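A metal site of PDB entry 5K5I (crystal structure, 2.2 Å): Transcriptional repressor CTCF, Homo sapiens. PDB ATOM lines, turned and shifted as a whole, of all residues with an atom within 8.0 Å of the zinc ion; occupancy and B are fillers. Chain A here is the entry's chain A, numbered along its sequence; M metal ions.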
ATOM      1  N   LYS A  96     -24.780  -4.778  19.298  1.00  0.00           N
ATOM      2  CA  LYS A  96     -23.597  -4.372  20.053  1.00  0.00           C
ATOM      3  C   LYS A  96     -22.819  -5.590  20.534  1.00  0.00           C
ATOM      4  O   LYS A  96     -23.374  -6.662  20.774  1.00  0.00           O
ATOM      5  CB  LYS A  96     -24.009  -3.507  21.246  1.00  0.00           C
ATOM      6  CG  LYS A  96     -24.817  -2.280  20.868  1.00  0.00           C
ATOM      7  CD  LYS A  96     -25.238  -1.501  22.102  1.00  0.00           C
ATOM      8  CE  LYS A  96     -26.082  -0.282  21.725  1.00  0.00           C
ATOM      9  NZ  LYS A  96     -26.502   0.488  22.923  1.00  0.00           N
ATOM     10  N   CYS A  97     -21.503  -5.407  20.661  1.00  0.00           N
ATOM     11  CA  CYS A  97     -20.651  -6.484  21.159  1.00  0.00           C
ATOM     12  C   CYS A  97     -20.989  -6.795  22.608  1.00  0.00           C
ATOM     13  O   CYS A  97     -21.348  -5.902  23.387  1.00  0.00           O
ATOM     14  CB  CYS A  97     -19.181  -6.089  21.035  1.00  0.00           C
ATOM     15  SG  CYS A  97     -18.020  -7.312  21.685  1.00  0.00           S
ATOM     16  N   ARG A  98     -20.891  -8.072  22.970  1.00  0.00           N
ATOM     17  CA  ARG A  98     -21.202  -8.486  24.329  1.00  0.00           C
ATOM     18  C   ARG A  98     -20.234  -7.896  25.350  1.00  0.00           C
ATOM     19  O   ARG A  98     -20.612  -7.670  26.504  1.00  0.00           O
ATOM     20  CB  ARG A  98     -21.207 -10.016  24.429  1.00  0.00           C
ATOM     21  CG  ARG A  98     -22.168 -10.690  23.475  1.00  0.00           C
ATOM     22  CD  ARG A  98     -22.026 -12.202  23.523  1.00  0.00           C
ATOM     23  NE  ARG A  98     -22.812 -12.861  22.487  1.00  0.00           N
ATOM     24  CZ  ARG A  98     -22.821 -14.173  22.272  1.00  0.00           C
ATOM     25  NH1 ARG A  98     -22.073 -14.976  23.011  1.00  0.00           N
ATOM     26  NH2 ARG A  98     -23.574 -14.683  21.304  1.00  0.00           N
ATOM     27  N   TYR A  99     -18.994  -7.629  24.937  1.00  0.00           N
ATOM     28  CA  TYR A  99     -17.971  -7.103  25.832  1.00  0.00           C
ATOM     29  C   TYR A  99     -17.768  -5.605  25.664  1.00  0.00           C
ATOM     30  O   TYR A  99     -17.897  -4.838  26.632  1.00  0.00           O
ATOM     31  CB  TYR A  99     -16.647  -7.853  25.612  1.00  0.00           C
ATOM     32  CG  TYR A  99     -16.736  -9.337  25.894  1.00  0.00           C
ATOM     33  CD1 TYR A  99     -16.470  -9.834  27.170  1.00  0.00           C
ATOM     34  CD2 TYR A  99     -17.087 -10.242  24.901  1.00  0.00           C
ATOM     35  CE1 TYR A  99     -16.542 -11.190  27.437  1.00  0.00           C
ATOM     36  CE2 TYR A  99     -17.164 -11.599  25.160  1.00  0.00           C
ATOM     37  CZ  TYR A  99     -16.898 -12.064  26.431  1.00  0.00           C
ATOM     38  OH  TYR A  99     -16.972 -13.411  26.699  1.00  0.00           O
ATOM     39  N   CYS A 100     -17.445  -5.152  24.461  1.00  0.00           N
ATOM     40  CA  CYS A 100     -17.175  -3.757  24.189  1.00  0.00           C
ATOM     41  C   CYS A 100     -18.381  -3.120  23.499  1.00  0.00           C
ATOM     42  O   CYS A 100     -19.432  -3.732  23.334  1.00  0.00           O
ATOM     43  CB  CYS A 100     -15.892  -3.609  23.364  1.00  0.00           C
ATOM     44  SG  CYS A 100     -15.956  -4.378  21.727  1.00  0.00           S
ATOM     45  N   ASP A 101     -18.219  -1.860  23.075  1.00  0.00           N
ATOM     46  CA  ASP A 101     -19.276  -1.106  22.428  1.00  0.00           C
ATOM     47  C   ASP A 101     -19.271  -1.234  20.905  1.00  0.00           C
ATOM     48  O   ASP A 101     -20.009  -0.524  20.232  1.00  0.00           O
ATOM     49  CB  ASP A 101     -19.185   0.376  22.808  1.00  0.00           C
ATOM     50  CG  ASP A 101     -19.501   0.615  24.270  1.00  0.00           C
ATOM     51  OD1 ASP A 101     -19.283  -0.298  25.085  1.00  0.00           O
ATOM     52  OD2 ASP A 101     -19.965   1.726  24.608  1.00  0.00           O
ATOM     53  N   ALA A 102     -18.427  -2.120  20.358  1.00  0.00           N
ATOM     54  CA  ALA A 102     -18.368  -2.289  18.914  1.00  0.00           C
ATOM     55  C   ALA A 102     -19.685  -2.839  18.375  1.00  0.00           C
ATOM     56  O   ALA A 102     -20.349  -3.664  19.019  1.00  0.00           O
ATOM     57  CB  ALA A 102     -17.220  -3.221  18.532  1.00  0.00           C
ATOM     58  N   VAL A 103     -20.060  -2.382  17.177  1.00  0.00           N
ATOM     59  CA  VAL A 103     -21.317  -2.759  16.541  1.00  0.00           C
ATOM     60  C   VAL A 103     -21.010  -3.355  15.179  1.00  0.00           C
ATOM     61  O   VAL A 103     -20.117  -2.884  14.475  1.00  0.00           O
ATOM     62  CB  VAL A 103     -22.269  -1.545  16.418  1.00  0.00           C
ATOM     63  CG1 VAL A 103     -23.618  -1.988  15.875  1.00  0.00           C
ATOM     64  CG2 VAL A 103     -22.434  -0.852  17.770  1.00  0.00           C
ATOM     65  N   PHE A 104     -21.765  -4.391  14.809  1.00  0.00           N
ATOM     66  CA  PHE A 104     -21.566  -5.078  13.543  1.00  0.00           C
ATOM     67  C   PHE A 104     -22.909  -5.362  12.891  1.00  0.00           C
ATOM     68  O   PHE A 104     -23.884  -5.698  13.584  1.00  0.00           O
ATOM     69  CB  PHE A 104     -20.790  -6.389  13.735  1.00  0.00           C
ATOM     70  CG  PHE A 104     -19.408  -6.196  14.300  1.00  0.00           C
ATOM     71  CD1 PHE A 104     -18.326  -6.034  13.461  1.00  0.00           C
ATOM     72  CD2 PHE A 104     -19.200  -6.185  15.671  1.00  0.00           C
ATOM     73  CE1 PHE A 104     -17.057  -5.846  13.969  1.00  0.00           C
ATOM     74  CE2 PHE A 104     -17.937  -6.009  16.184  1.00  0.00           C
ATOM     75  CZ  PHE A 104     -16.863  -5.839  15.338  1.00  0.00           C
ATOM     76  N   LEU A 110     -19.588 -10.269  13.774  1.00  0.00           N
ATOM     77  CA  LEU A 110     -19.833 -10.052  15.203  1.00  0.00           C
ATOM     78  C   LEU A 110     -19.222 -11.169  16.037  1.00  0.00           C
ATOM     79  O   LEU A 110     -18.551 -10.908  17.042  1.00  0.00           O
ATOM     80  CB  LEU A 110     -21.337  -9.955  15.469  1.00  0.00           C
ATOM     81  CG  LEU A 110     -21.761  -9.824  16.931  1.00  0.00           C
ATOM     82  CD1 LEU A 110     -21.209  -8.548  17.550  1.00  0.00           C
ATOM     83  CD2 LEU A 110     -23.274  -9.879  17.053  1.00  0.00           C
ATOM     84  N   GLN A 112     -16.817 -13.279  15.158  1.00  0.00           N
ATOM     85  CA  GLN A 112     -15.365 -13.309  15.004  1.00  0.00           C
ATOM     86  C   GLN A 112     -14.685 -12.248  15.867  1.00  0.00           C
ATOM     87  O   GLN A 112     -13.566 -12.466  16.345  1.00  0.00           O
ATOM     88  CB  GLN A 112     -14.986 -13.121  13.531  1.00  0.00           C
ATOM     89  CG  GLN A 112     -14.026 -14.176  13.012  1.00  0.00           C
ATOM     90  CD  GLN A 112     -14.638 -15.572  13.029  1.00  0.00           C
ATOM     91  OE1 GLN A 112     -15.802 -15.752  12.691  1.00  0.00           O
ATOM     92  NE2 GLN A 112     -13.848 -16.558  13.436  1.00  0.00           N
ATOM     93  N   HIS A 113     -15.345 -11.109  16.078  1.00  0.00           N
ATOM     94  CA  HIS A 113     -14.786 -10.088  16.967  1.00  0.00           C
ATOM     95  C   HIS A 113     -14.921 -10.483  18.424  1.00  0.00           C
ATOM     96  O   HIS A 113     -14.012 -10.239  19.225  1.00  0.00           O
ATOM     97  CB  HIS A 113     -15.455  -8.738  16.711  1.00  0.00           C
ATOM     98  CG  HIS A 113     -15.158  -7.704  17.747  1.00  0.00           C
ATOM     99  ND1 HIS A 113     -13.916  -7.106  17.859  1.00  0.00           N
ATOM    100  CD2 HIS A 113     -15.922  -7.175  18.734  1.00  0.00           C
ATOM    101  CE1 HIS A 113     -13.942  -6.243  18.867  1.00  0.00           C
ATOM    102  NE2 HIS A 113     -15.146  -6.269  19.407  1.00  0.00           N
ATOM    103  N   GLN A 114     -16.061 -11.075  18.799  1.00  0.00           N
ATOM    104  CA  GLN A 114     -16.247 -11.511  20.187  1.00  0.00           C
ATOM    105  C   GLN A 114     -15.241 -12.597  20.560  1.00  0.00           C
ATOM    106  O   GLN A 114     -14.755 -12.634  21.703  1.00  0.00           O
ATOM    107  CB  GLN A 114     -17.673 -12.001  20.390  1.00  0.00           C
ATOM    108  CG  GLN A 114     -18.728 -10.915  20.267  1.00  0.00           C
ATOM    109  CD  GLN A 114     -20.140 -11.452  20.419  1.00  0.00           C
ATOM    110  OE1 GLN A 114     -20.344 -12.642  20.632  1.00  0.00           O
ATOM    111  NE2 GLN A 114     -21.123 -10.555  20.308  1.00  0.00           N
ATOM    112  N   LYS A 115     -14.920 -13.484  19.624  1.00  0.00           N
ATOM    113  CA  LYS A 115     -13.914 -14.504  19.880  1.00  0.00           C
ATOM    114  C   LYS A 115     -12.516 -13.899  20.019  1.00  0.00           C
ATOM    115  O   LYS A 115     -11.625 -14.547  20.595  1.00  0.00           O
ATOM    116  CB  LYS A 115     -13.919 -15.556  18.771  1.00  0.00           C
ATOM    117  CG  LYS A 115     -15.168 -16.417  18.746  1.00  0.00           C
ATOM    118  CD  LYS A 115     -15.079 -17.478  17.660  1.00  0.00           C
ATOM    119  CE  LYS A 115     -16.302 -18.385  17.672  1.00  0.00           C
ATOM    120  NZ  LYS A 115     -16.223 -19.440  16.628  1.00  0.00           N
ATOM    121  N   SER A 116     -12.299 -12.694  19.492  1.00  0.00           N
ATOM    122  CA  SER A 116     -10.999 -12.040  19.619  1.00  0.00           C
ATOM    123  C   SER A 116     -10.740 -11.524  21.025  1.00  0.00           C
ATOM    124  O   SER A 116      -9.603 -11.133  21.317  1.00  0.00           O
ATOM    125  CB  SER A 116     -10.897 -10.887  18.620  1.00  0.00           C
ATOM    126  OG  SER A 116      -9.643 -10.234  18.716  1.00  0.00           O
ATOM    127  N   HIS A 117     -11.739 -11.502  21.893  1.00  0.00           N
ATOM    128  CA  HIS A 117     -11.555 -11.054  23.273  1.00  0.00           C
ATOM    129  C   HIS A 117     -11.113 -12.205  24.175  1.00  0.00           C
ATOM    130  O   HIS A 117      -9.976 -12.675  24.081  1.00  0.00           O
ATOM    131  CB  HIS A 117     -12.849 -10.442  23.805  1.00  0.00           C
ATOM    132  CG  HIS A 117     -13.241  -9.164  23.131  1.00  0.00           C
ATOM    133  ND1 HIS A 117     -12.332  -8.371  22.450  1.00  0.00           N
ATOM    134  CD2 HIS A 117     -14.432  -8.525  23.035  1.00  0.00           C
ATOM    135  CE1 HIS A 117     -12.947  -7.308  21.964  1.00  0.00           C
ATOM    136  NE2 HIS A 117     -14.225  -7.386  22.306  1.00  0.00           N
HETATM  137 ZN    ZN M   1     -15.826  -6.628  21.296  1.00  0.00          ZN
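The nearest printed residue that does not touch the zinc ion is Tyr 99 (4.6 Å).
The backbone carbonyl oxygen of Ala 102 is in hydrogen-bond range of the backbone NH of Cys 97. The backbone NH (N) of Ala 102 lies close to the side-chain sulfur (SG) of Cys 100, at 3.6 Å. The side-chain sulfur of Cys 97 lies close to the backbone NH of Tyr 99 (3.4 Å).
The zinc ion is bound by NE2 of His 117 (2.0 Å), NE2 of His 113 (2.0 Å), SG of Cys 100 (2.3 Å) and SG of Cys 97 (2.3 Å).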
